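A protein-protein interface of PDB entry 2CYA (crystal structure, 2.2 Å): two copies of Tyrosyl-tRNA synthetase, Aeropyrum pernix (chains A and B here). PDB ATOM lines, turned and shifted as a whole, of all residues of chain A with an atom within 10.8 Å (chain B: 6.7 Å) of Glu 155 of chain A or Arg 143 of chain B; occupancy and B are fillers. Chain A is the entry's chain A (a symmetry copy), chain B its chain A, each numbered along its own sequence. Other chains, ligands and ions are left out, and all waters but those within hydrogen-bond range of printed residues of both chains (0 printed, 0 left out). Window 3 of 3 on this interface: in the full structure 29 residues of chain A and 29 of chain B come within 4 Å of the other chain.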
ATOM      1  N   SER A 138     -14.597  13.067 -24.254  1.00  0.00           N
ATOM      2  CA  SER A 138     -15.997  13.460 -24.338  1.00  0.00           C
ATOM      3  C   SER A 138     -16.886  12.286 -24.718  1.00  0.00           C
ATOM      4  O   SER A 138     -16.410  11.277 -25.232  1.00  0.00           O
ATOM      5  CB  SER A 138     -16.164  14.588 -25.366  1.00  0.00           C
ATOM      6  OG  SER A 138     -15.994  14.108 -26.690  1.00  0.00           O
ATOM      7  N   LEU A 139     -18.181  12.416 -24.455  1.00  0.00           N
ATOM      8  CA  LEU A 139     -19.118  11.357 -24.797  1.00  0.00           C
ATOM      9  C   LEU A 139     -19.096  11.230 -26.318  1.00  0.00           C
ATOM     10  O   LEU A 139     -19.381  10.162 -26.873  1.00  0.00           O
ATOM     11  CB  LEU A 139     -20.530  11.713 -24.312  1.00  0.00           C
ATOM     12  CG  LEU A 139     -21.647  10.679 -24.526  1.00  0.00           C
ATOM     13  CD1 LEU A 139     -22.854  11.018 -23.649  1.00  0.00           C
ATOM     14  CD2 LEU A 139     -22.061  10.653 -25.985  1.00  0.00           C
ATOM     15  N   ALA A 140     -18.761  12.333 -26.984  1.00  0.00           N
ATOM     16  CA  ALA A 140     -18.688  12.345 -28.441  1.00  0.00           C
ATOM     17  C   ALA A 140     -17.438  11.578 -28.867  1.00  0.00           C
ATOM     18  O   ALA A 140     -17.514  10.663 -29.690  1.00  0.00           O
ATOM     19  CB  ALA A 140     -18.637  13.787 -28.966  1.00  0.00           C
ATOM     20  N   ARG A 141     -16.291  11.943 -28.300  1.00  0.00           N
ATOM     21  CA  ARG A 141     -15.048  11.257 -28.643  1.00  0.00           C
ATOM     22  C   ARG A 141     -15.225   9.755 -28.429  1.00  0.00           C
ATOM     23  O   ARG A 141     -14.879   8.954 -29.293  1.00  0.00           O
ATOM     24  CB  ARG A 141     -13.880  11.776 -27.794  1.00  0.00           C
ATOM     25  CG  ARG A 141     -12.551  11.066 -28.079  1.00  0.00           C
ATOM     26  CD  ARG A 141     -12.072  11.350 -29.498  1.00  0.00           C
ATOM     27  NE  ARG A 141     -10.980  10.474 -29.934  1.00  0.00           N
ATOM     28  CZ  ARG A 141     -11.149   9.231 -30.380  1.00  0.00           C
ATOM     29  NH1 ARG A 141     -12.363   8.700 -30.442  1.00  0.00           N
ATOM     30  NH2 ARG A 141     -10.107   8.533 -30.812  1.00  0.00           N
ATOM     31  N   ARG A 143     -18.027   8.162 -28.295  1.00  0.00           N
ATOM     32  CA  ARG A 143     -19.077   7.634 -29.150  1.00  0.00           C
ATOM     33  C   ARG A 143     -18.564   7.351 -30.557  1.00  0.00           C
ATOM     34  O   ARG A 143     -19.041   6.429 -31.222  1.00  0.00           O
ATOM     35  CB  ARG A 143     -20.263   8.598 -29.196  1.00  0.00           C
ATOM     36  CG  ARG A 143     -21.574   7.930 -29.577  1.00  0.00           C
ATOM     37  CD  ARG A 143     -22.763   8.816 -29.240  1.00  0.00           C
ATOM     38  NE  ARG A 143     -24.033   8.187 -29.581  1.00  0.00           N
ATOM     39  CZ  ARG A 143     -25.221   8.742 -29.366  1.00  0.00           C
ATOM     40  NH1 ARG A 143     -25.301   9.946 -28.807  1.00  0.00           N
ATOM     41  NH2 ARG A 143     -26.330   8.095 -29.703  1.00  0.00           N
ATOM     42  N   LEU A 146     -17.239   3.783 -31.153  1.00  0.00           N
ATOM     43  CA  LEU A 146     -18.163   2.658 -31.124  1.00  0.00           C
ATOM     44  C   LEU A 146     -18.369   2.156 -32.543  1.00  0.00           C
ATOM     45  O   LEU A 146     -18.726   2.936 -33.424  1.00  0.00           O
ATOM     46  CB  LEU A 146     -19.509   3.093 -30.552  1.00  0.00           C
ATOM     47  CG  LEU A 146     -19.494   3.823 -29.208  1.00  0.00           C
ATOM     48  CD1 LEU A 146     -20.931   4.095 -28.784  1.00  0.00           C
ATOM     49  CD2 LEU A 146     -18.775   2.987 -28.158  1.00  0.00           C
ATOM     50  N   ALA A 153     -26.635   5.606 -34.532  1.00  0.00           N
ATOM     51  CA  ALA A 153     -27.362   5.009 -33.416  1.00  0.00           C
ATOM     52  C   ALA A 153     -27.767   6.078 -32.406  1.00  0.00           C
ATOM     53  O   ALA A 153     -26.910   6.689 -31.766  1.00  0.00           O
ATOM     54  CB  ALA A 153     -26.497   3.947 -32.737  1.00  0.00           C
ATOM     55  N   GLU A 154     -29.069   6.306 -32.263  1.00  0.00           N
ATOM     56  CA  GLU A 154     -29.547   7.308 -31.318  1.00  0.00           C
ATOM     57  C   GLU A 154     -29.499   6.796 -29.880  1.00  0.00           C
ATOM     58  O   GLU A 154     -29.647   5.601 -29.623  1.00  0.00           O
ATOM     59  CB  GLU A 154     -30.966   7.762 -31.684  1.00  0.00           C
ATOM     60  CG  GLU A 154     -31.929   6.635 -32.018  1.00  0.00           C
ATOM     61  CD  GLU A 154     -33.258   7.145 -32.561  1.00  0.00           C
ATOM     62  OE1 GLU A 154     -33.239   7.949 -33.521  1.00  0.00           O
ATOM     63  OE2 GLU A 154     -34.317   6.738 -32.033  1.00  0.00           O
ATOM     64  N   GLU A 155     -29.282   7.722 -28.953  1.00  0.00           N
ATOM     65  CA  GLU A 155     -29.175   7.430 -27.528  1.00  0.00           C
ATOM     66  C   GLU A 155     -30.092   6.346 -26.959  1.00  0.00           C
ATOM     67  O   GLU A 155     -29.646   5.494 -26.192  1.00  0.00           O
ATOM     68  CB  GLU A 155     -29.369   8.721 -26.731  1.00  0.00           C
ATOM     69  CG  GLU A 155     -28.276   9.755 -26.946  1.00  0.00           C
ATOM     70  CD  GLU A 155     -28.498  11.013 -26.124  1.00  0.00           C
ATOM     71  OE1 GLU A 155     -28.777  10.888 -24.914  1.00  0.00           O
ATOM     72  OE2 GLU A 155     -28.391  12.127 -26.679  1.00  0.00           O
ATOM     73  N   ALA A 156     -31.364   6.369 -27.338  1.00  0.00           N
ATOM     74  CA  ALA A 156     -32.336   5.404 -26.819  1.00  0.00           C
ATOM     75  C   ALA A 156     -32.125   3.927 -27.169  1.00  0.00           C
ATOM     76  O   ALA A 156     -32.839   3.065 -26.647  1.00  0.00           O
ATOM     77  CB  ALA A 156     -33.740   5.832 -27.232  1.00  0.00           C
ATOM     78  N   GLU A 157     -31.158   3.624 -28.035  1.00  0.00           N
ATOM     79  CA  GLU A 157     -30.902   2.233 -28.433  1.00  0.00           C
ATOM     80  C   GLU A 157     -29.543   1.709 -27.975  1.00  0.00           C
ATOM     81  O   GLU A 157     -29.326   0.498 -27.910  1.00  0.00           O
ATOM     82  CB  GLU A 157     -30.995   2.087 -29.957  1.00  0.00           C
ATOM     83  CG  GLU A 157     -32.349   2.438 -30.541  1.00  0.00           C
ATOM     84  CD  GLU A 157     -33.459   1.569 -29.984  1.00  0.00           C
ATOM     85  OE1 GLU A 157     -33.371   0.327 -30.120  1.00  0.00           O
ATOM     86  OE2 GLU A 157     -34.419   2.132 -29.410  1.00  0.00           O
ATOM     87  N   VAL A 158     -28.633   2.628 -27.670  1.00  0.00           N
ATOM     88  CA  VAL A 158     -27.286   2.276 -27.227  1.00  0.00           C
ATOM     89  C   VAL A 158     -27.216   2.188 -25.701  1.00  0.00           C
ATOM     90  O   VAL A 158     -27.143   3.220 -25.032  1.00  0.00           O
ATOM     91  CB  VAL A 158     -26.262   3.341 -27.684  1.00  0.00           C
ATOM     92  CG1 VAL A 158     -24.850   2.846 -27.434  1.00  0.00           C
ATOM     93  CG2 VAL A 158     -26.474   3.675 -29.150  1.00  0.00           C
ATOM     94  N   ASP A 159     -27.226   0.978 -25.147  1.00  0.00           N
ATOM     95  CA  ASP A 159     -27.155   0.858 -23.694  1.00  0.00           C
ATOM     96  C   ASP A 159     -25.788   1.337 -23.202  1.00  0.00           C
ATOM     97  O   ASP A 159     -24.777   1.159 -23.884  1.00  0.00           O
ATOM     98  CB  ASP A 159     -27.453  -0.581 -23.236  1.00  0.00           C
ATOM     99  CG  ASP A 159     -26.344  -1.554 -23.554  1.00  0.00           C
ATOM    100  OD1 ASP A 159     -25.996  -1.721 -24.741  1.00  0.00           O
ATOM    101  OD2 ASP A 159     -25.827  -2.170 -22.601  1.00  0.00           O
ATOM    102  N   ALA A 160     -25.785   1.977 -22.031  1.00  0.00           N
ATOM    103  CA  ALA A 160     -24.582   2.544 -21.420  1.00  0.00           C
ATOM    104  C   ALA A 160     -23.350   1.643 -21.331  1.00  0.00           C
ATOM    105  O   ALA A 160     -22.224   2.129 -21.404  1.00  0.00           O
ATOM    106  CB  ALA A 160     -24.925   3.088 -20.023  1.00  0.00           C
ATOM    107  N   SER A 161     -23.549   0.344 -21.163  1.00  0.00           N
ATOM    108  CA  SER A 161     -22.418  -0.562 -21.068  1.00  0.00           C
ATOM    109  C   SER A 161     -21.559  -0.516 -22.340  1.00  0.00           C
ATOM    110  O   SER A 161     -20.380  -0.872 -22.313  1.00  0.00           O
ATOM    111  CB  SER A 161     -22.912  -1.984 -20.800  1.00  0.00           C
ATOM    112  OG  SER A 161     -23.632  -2.482 -21.908  1.00  0.00           O
ATOM    113  N   LYS A 162     -22.139  -0.047 -23.443  1.00  0.00           N
ATOM    114  CA  LYS A 162     -21.420   0.044 -24.712  1.00  0.00           C
ATOM    115  C   LYS A 162     -20.396   1.160 -24.695  1.00  0.00           C
ATOM    116  O   LYS A 162     -19.439   1.138 -25.467  1.00  0.00           O
ATOM    117  CB  LYS A 162     -22.382   0.277 -25.887  1.00  0.00           C
ATOM    118  CG  LYS A 162     -23.457  -0.780 -26.056  1.00  0.00           C
ATOM    119  CD  LYS A 162     -22.874  -2.128 -26.425  1.00  0.00           C
ATOM    120  CE  LYS A 162     -23.975  -3.133 -26.738  1.00  0.00           C
ATOM    121  NZ  LYS A 162     -23.408  -4.389 -27.291  1.00  0.00           N
ATOM    122  N   LEU A 163     -20.604   2.154 -23.839  1.00  0.00           N
ATOM    123  CA  LEU A 163     -19.655   3.254 -23.732  1.00  0.00           C
ATOM    124  C   LEU A 163     -18.533   2.853 -22.784  1.00  0.00           C
ATOM    125  O   LEU A 163     -17.405   3.317 -22.909  1.00  0.00           O
ATOM    126  CB  LEU A 163     -20.332   4.526 -23.215  1.00  0.00           C
ATOM    127  CG  LEU A 163     -20.840   5.509 -24.280  1.00  0.00           C
ATOM    128  CD1 LEU A 163     -21.912   4.850 -25.151  1.00  0.00           C
ATOM    129  CD2 LEU A 163     -21.390   6.745 -23.587  1.00  0.00           C
ATOM    130  N   SER B 138     -30.330   2.661 -21.205  1.00  0.00           N
ATOM    131  CA  SER B 138     -29.865   3.299 -22.430  1.00  0.00           C
ATOM    132  C   SER B 138     -29.037   4.540 -22.133  1.00  0.00           C
ATOM    133  O   SER B 138     -29.095   5.089 -21.036  1.00  0.00           O
ATOM    134  CB  SER B 138     -31.065   3.678 -23.310  1.00  0.00           C
ATOM    135  OG  SER B 138     -31.787   4.767 -22.758  1.00  0.00           O
ATOM    136  N   LEU B 139     -28.256   4.977 -23.115  1.00  0.00           N
ATOM    137  CA  LEU B 139     -27.438   6.167 -22.939  1.00  0.00           C
ATOM    138  C   LEU B 139     -28.401   7.332 -22.734  1.00  0.00           C
ATOM    139  O   LEU B 139     -28.061   8.338 -22.100  1.00  0.00           O
ATOM    140  CB  LEU B 139     -26.566   6.407 -24.179  1.00  0.00           C
ATOM    141  CG  LEU B 139     -25.581   7.587 -24.150  1.00  0.00           C
ATOM    142  CD1 LEU B 139     -24.545   7.436 -25.265  1.00  0.00           C
ATOM    143  CD2 LEU B 139     -26.331   8.895 -24.316  1.00  0.00           C
ATOM    144  N   ALA B 140     -29.606   7.188 -23.282  1.00  0.00           N
ATOM    145  CA  ALA B 140     -30.627   8.221 -23.150  1.00  0.00           C
ATOM    146  C   ALA B 140     -31.158   8.195 -21.718  1.00  0.00           C
ATOM    147  O   ALA B 140     -31.185   9.224 -21.041  1.00  0.00           O
ATOM    148  CB  ALA B 140     -31.768   7.981 -24.149  1.00  0.00           C
ATOM    149  N   ARG B 141     -31.567   7.016 -21.254  1.00  0.00           N
ATOM    150  CA  ARG B 141     -32.080   6.898 -19.893  1.00  0.00           C
ATOM    151  C   ARG B 141     -31.050   7.460 -18.914  1.00  0.00           C
ATOM    152  O   ARG B 141     -31.386   8.250 -18.036  1.00  0.00           O
ATOM    153  CB  ARG B 141     -32.393   5.436 -19.547  1.00  0.00           C
ATOM    154  CG  ARG B 141     -32.900   5.240 -18.114  1.00  0.00           C
ATOM    155  CD  ARG B 141     -34.251   5.916 -17.912  1.00  0.00           C
ATOM    156  NE  ARG B 141     -34.648   6.027 -16.505  1.00  0.00           N
ATOM    157  CZ  ARG B 141     -34.201   6.964 -15.671  1.00  0.00           C
ATOM    158  NH1 ARG B 141     -33.330   7.874 -16.089  1.00  0.00           N
ATOM    159  NH2 ARG B 141     -34.664   7.022 -14.429  1.00  0.00           N
ATOM    160  N   VAL B 142     -29.790   7.066 -19.090  1.00  0.00           N
ATOM    161  CA  VAL B 142     -28.710   7.533 -18.225  1.00  0.00           C
ATOM    162  C   VAL B 142     -28.443   9.013 -18.416  1.00  0.00           C
ATOM    163  O   VAL B 142     -28.048   9.707 -17.487  1.00  0.00           O
ATOM    164  CB  VAL B 142     -27.384   6.774 -18.497  1.00  0.00           C
ATOM    165  CG1 VAL B 142     -26.246   7.410 -17.703  1.00  0.00           C
ATOM    166  CG2 VAL B 142     -27.534   5.305 -18.118  1.00  0.00           C
ATOM    167  N   ARG B 143     -28.660   9.507 -19.624  1.00  0.00           N
ATOM    168  CA  ARG B 143     -28.408  10.914 -19.884  1.00  0.00           C
ATOM    169  C   ARG B 143     -29.469  11.801 -19.242  1.00  0.00           C
ATOM    170  O   ARG B 143     -29.179  12.928 -18.838  1.00  0.00           O
ATOM    171  CB  ARG B 143     -28.332  11.174 -21.389  1.00  0.00           C
ATOM    172  CG  ARG B 143     -27.552  12.428 -21.750  1.00  0.00           C
ATOM    173  CD  ARG B 143     -27.177  12.438 -23.224  1.00  0.00           C
ATOM    174  NE  ARG B 143     -26.411  13.624 -23.588  1.00  0.00           N
ATOM    175  CZ  ARG B 143     -25.943  13.862 -24.809  1.00  0.00           C
ATOM    176  NH1 ARG B 143     -26.164  12.990 -25.788  1.00  0.00           N
ATOM    177  NH2 ARG B 143     -25.250  14.967 -25.053  1.00  0.00           N
ATOM    178  N   ARG B 144     -30.698  11.308 -19.132  1.00  0.00           N
ATOM    179  CA  ARG B 144     -31.720  12.136 -18.513  1.00  0.00           C
ATOM    180  C   ARG B 144     -31.633  12.027 -16.992  1.00  0.00           C
ATOM    181  O   ARG B 144     -32.536  12.449 -16.275  1.00  0.00           O
ATOM    182  CB  ARG B 144     -33.132  11.785 -19.035  1.00  0.00           C
ATOM    183  CG  ARG B 144     -33.807  10.537 -18.483  1.00  0.00           C
ATOM    184  CD  ARG B 144     -35.194  10.375 -19.126  1.00  0.00           C
ATOM    185  NE  ARG B 144     -35.910   9.177 -18.684  1.00  0.00           N
ATOM    186  CZ  ARG B 144     -36.537   9.049 -17.512  1.00  0.00           C
ATOM    187  NH1 ARG B 144     -36.552  10.049 -16.635  1.00  0.00           N
ATOM    188  NH2 ARG B 144     -37.151   7.910 -17.215  1.00  0.00           N
ATOM    189  N   ALA B 145     -30.524  11.469 -16.513  1.00  0.00           N
ATOM    190  CA  ALA B 145     -30.279  11.325 -15.080  1.00  0.00           C
ATOM    191  C   ALA B 145     -29.122  12.245 -14.706  1.00  0.00           C
ATOM    192  O   ALA B 145     -28.648  12.242 -13.574  1.00  0.00           O
ATOM    193  CB  ALA B 145     -29.935   9.878 -14.735  1.00  0.00           C
ATOM    194  N   LEU B 146     -28.670  13.027 -15.679  1.00  0.00           N
ATOM    195  CA  LEU B 146     -27.575  13.964 -15.469  1.00  0.00           C
ATOM    196  C   LEU B 146     -28.153  15.331 -15.146  1.00  0.00           C
ATOM    197  O   LEU B 146     -28.971  15.846 -15.906  1.00  0.00           O
ATOM    198  CB  LEU B 146     -26.721  14.071 -16.729  1.00  0.00           C
ATOM    199  CG  LEU B 146     -26.214  12.766 -17.343  1.00  0.00           C
ATOM    200  CD1 LEU B 146     -25.326  13.099 -18.534  1.00  0.00           C
ATOM    201  CD2 LEU B 146     -25.442  11.958 -16.309  1.00  0.00           C
ATOM    202  N   ALA B 153     -27.013  19.737 -23.113  1.00  0.00           N
ATOM    203  CA  ALA B 153     -25.571  19.545 -23.230  1.00  0.00           C
ATOM    204  C   ALA B 153     -25.248  18.567 -24.355  1.00  0.00           C
ATOM    205  O   ALA B 153     -25.588  17.385 -24.272  1.00  0.00           O
ATOM    206  CB  ALA B 153     -25.003  19.028 -21.908  1.00  0.00           C
ATOM    207  N   GLU B 154     -24.595  19.055 -25.406  1.00  0.00           N
ATOM    208  CA  GLU B 154     -24.243  18.192 -26.527  1.00  0.00           C
ATOM    209  C   GLU B 154     -23.033  17.317 -26.206  1.00  0.00           C
ATOM    210  O   GLU B 154     -22.151  17.703 -25.439  1.00  0.00           O
ATOM    211  CB  GLU B 154     -23.990  19.024 -27.790  1.00  0.00           C
ATOM    212  CG  GLU B 154     -23.117  20.249 -27.581  1.00  0.00           C
ATOM    213  CD  GLU B 154     -23.060  21.141 -28.816  1.00  0.00           C
ATOM    214  OE1 GLU B 154     -24.139  21.506 -29.337  1.00  0.00           O
ATOM    215  OE2 GLU B 154     -21.939  21.481 -29.258  1.00  0.00           O
ATOM    216  N   GLU B 155     -23.015  16.131 -26.804  1.00  0.00           N
ATOM    217  CA  GLU B 155     -21.960  15.142 -26.606  1.00  0.00           C
ATOM    218  C   GLU B 155     -20.528  15.659 -26.456  1.00  0.00           C
ATOM    219  O   GLU B 155     -19.795  15.210 -25.575  1.00  0.00           O
ATOM    220  CB  GLU B 155     -22.008  14.117 -27.741  1.00  0.00           C
ATOM    221  CG  GLU B 155     -23.267  13.268 -27.759  1.00  0.00           C
ATOM    222  CD  GLU B 155     -23.266  12.253 -28.889  1.00  0.00           C
ATOM    223  OE1 GLU B 155     -22.244  11.558 -29.061  1.00  0.00           O
ATOM    224  OE2 GLU B 155     -24.283  12.143 -29.607  1.00  0.00           O
ATOM    225  N   ALA B 156     -20.132  16.602 -27.302  1.00  0.00           N
ATOM    226  CA  ALA B 156     -18.769  17.135 -27.273  1.00  0.00           C
ATOM    227  C   ALA B 156     -18.331  17.898 -26.018  1.00  0.00           C
ATOM    228  O   ALA B 156     -17.154  18.248 -25.892  1.00  0.00           O
ATOM    229  CB  ALA B 156     -18.542  18.004 -28.504  1.00  0.00           C
ATOM    230  N   VAL B 158     -19.797  16.962 -22.684  1.00  0.00           N
ATOM    231  CA  VAL B 158     -20.014  16.069 -21.548  1.00  0.00           C
ATOM    232  C   VAL B 158     -18.981  14.940 -21.533  1.00  0.00           C
ATOM    233  O   VAL B 158     -19.116  13.977 -22.289  1.00  0.00           O
ATOM    234  CB  VAL B 158     -21.416  15.421 -21.621  1.00  0.00           C
ATOM    235  CG1 VAL B 158     -21.722  14.695 -20.324  1.00  0.00           C
ATOM    236  CG2 VAL B 158     -22.467  16.477 -21.917  1.00  0.00           C
ATOM    237  N   LEU B 163     -21.153  10.080 -17.193  1.00  0.00           N
ATOM    238  CA  LEU B 163     -22.158   9.041 -17.375  1.00  0.00           C
ATOM    239  C   LEU B 163     -21.893   7.913 -16.387  1.00  0.00           C
ATOM    240  O   LEU B 163     -22.809   7.216 -15.965  1.00  0.00           O
ATOM    241  CB  LEU B 163     -22.131   8.486 -18.803  1.00  0.00           C
ATOM    242  CG  LEU B 163     -23.102   9.132 -19.803  1.00  0.00           C
ATOM    243  CD1 LEU B 163     -22.779  10.618 -19.980  1.00  0.00           C
ATOM    244  CD2 LEU B 163     -23.004   8.396 -21.129  1.00  0.00           C
ATOM    245  N   LYS B 189     -32.636  12.445  -9.432  1.00  0.00           N
ATOM    246  CA  LYS B 189     -32.511  11.779 -10.719  1.00  0.00           C
ATOM    247  C   LYS B 189     -31.761  10.450 -10.612  1.00  0.00           C
ATOM    248  O   LYS B 189     -32.171   9.455 -11.196  1.00  0.00           O
ATOM    249  CB  LYS B 189     -31.854  12.711 -11.729  1.00  0.00           C
ATOM    250  CG  LYS B 189     -32.822  13.745 -12.304  1.00  0.00           C
ATOM    251  CD  LYS B 189     -32.119  14.643 -13.318  1.00  0.00           C
ATOM    252  CE  LYS B 189     -33.109  15.559 -14.035  1.00  0.00           C
ATOM    253  NZ  LYS B 189     -32.414  16.488 -14.975  1.00  0.00           N
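The backbone NH (N) of Leu 139 of chain B lies within hydrogen-bond range of the backbone carbonyl oxygen (O) of Glu 155 of chain A (3.4 Å). The backbone NH of Leu 139 of chain B is in hydrogen-bond range of the backbone carbonyl oxygen of Val 158 of chain A (2.8 Å). O of Glu 155 of chain A lies within hydrogen-bond range of N of Ala 140 of chain B (3.4 Å). The side-chain carboxylate (OE2) of Glu 155 of chain A is in salt-bridge range of the guanidinium group (NH1) of Arg 143 of chain B (2.5 Å). O of Glu 155 of chain B lies within hydrogen-bond range of N of Leu 139 of chain A (3.4 Å). The backbone NH of Ala 140 of chain A lies within hydrogen-bond range of the backbone carbonyl oxygen of Glu 155 of chain B, 3.4 Å away. NH1 of Arg 143 of chain A is in salt-bridge range of OE2 of Glu 155 of chain B (2.6 Å). O of Val 158 of chain B lies within hydrogen-bond range of N of Leu 139 of chain A, 2.8 Å away.
The side-chain hydroxyl (OG) of Ser 138 of chain B lies close to the backbone NH (N) of Ala 140 of chain B, 3.3 Å away. OG of Ser 138 of chain B is in hydrogen-bond range of N of Arg 141 of chain B, 2.7 Å away. The guanidinium group of Arg 143 of chain B sits at hydrogen-bond distance from the backbone carbonyl oxygen of Ala 153 of chain B. N of Ala 140 of chain A sits close to OG of Ser 138 of chain A (3.3 Å). OG of Ser 138 of chain A lies within hydrogen-bond range of N of Arg 141 of chain A (2.7 Å). The guanidinium group (NH2) of Arg 143 of chain A lies within hydrogen-bond range of the backbone carbonyl oxygen (O) of Ala 153 of chain A, 2.6 Å away.
Glu 155 of chain A touches just these residues of chain B: Ser 138 (3.7 Å), Leu 139 (3.2 Å), Ala 140 (3.4 Å) and Arg 143 (2.5 Å). Arg 143 of chain B touches one residue of chain A. Of chain A, only Glu 155, Ala 156, Val 158 and Asp 159 come within 4 Å of Ser 138 of chain B. Ala 140 of chain B touches two residues of chain A. No residue of chain A comes within 4 Å of Ala 145 of chain B. Leu 146 of chain B touches none of the printed residues of chain A. No residue of chain A comes within 4 Å of Ala 153 of chain B. Of chain A, only Ser 138 (3.7 Å), Leu 139 (3.2 Å), Ala 140 (3.4 Å) and Arg 143 (2.6 Å) come within 4 Å of Glu 155 of chain B. Printed residues of chain B within 4 Å of Asp 159 of chain A: Ser 138 (3.9 Å). Of the printed residues of chain B, Leu 163 of chain A touches Leu 139 and Leu 163. Printed residues of chain A within 4 Å of Ala 156 of chain B: Ser 138 (3.8 Å) and Ala 140 (3.6 Å). Lys 189 of chain B touches none of the printed residues of chain A. Arg 141 of chain A touches none of the printed residues of chain B.
Of the 16 printed residues of chain B, 9 touch a printed residue of chain A. Hydrophobic or aromatic side chains of chain B within 4 Å of the printed part of chain A: Leu 139, Ala 140, Val 142 and Leu 163. Of the 17 printed residues of chain A, 10 touch a printed residue of chain B. Printed residues of chain A that touch a printed residue of chain B: Ser 138, Leu 139, Ala 140, Arg 143, Glu 155, Ala 156, Val 158, Asp 159, Ala 160 and Leu 163.
CB of Ser 138 of chain A touches O of Glu 155 of chain B, 3.7 Å away. Ser 138 of chain A touches Ala 156 of chain B (CB to O, 3.8 Å). Ser 138 of chain A touches Val 158 of chain B. Ala 140 of chain A touches Ala 156 of chain B. CB of Ser 138 of chain B touches O of Glu 155 of chain A, 3.7 Å away. O of Ala 156 of chain A touches CB of Ser 138 of chain B, at 3.8 Å. N of Ala 156 of chain A touches CB of Ala 140 of chain B (3.6 Å). Ala 160 of chain A touches Val 142 of chain B (CB to CG2, 3.9 Å). CD2 of Leu 163 of chain A touches CD1 of Leu 139 of chain B, at 3.6 Å. Leu 163 of chain A touches Leu 163 of chain B.
Ser 138 of chain A touches Ala 156 of chain B, and with the chains exchanged Ala 156 of chain A touches Ser 138 of chain B. Leu 139 of chain A touches Glu 155 of chain B, and with the chains exchanged Glu 155 of chain A touches Leu 139 of chain B. Ala 140 of chain A touches Ala 156 of chain B, and with the chains exchanged Ala 156 of chain A touches Ala 140 of chain B. Leu 163 of chain A touches its own counterpart, Leu 163 of chain B. Positions printed for both chains: 138, 139, 140, 141, 143, 146, 153, 154, 155, 156, 158 and 163. Of the 21 pairs that touch across the chains among the printed residues, 19 have their exchanged pair printed and touching as well.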
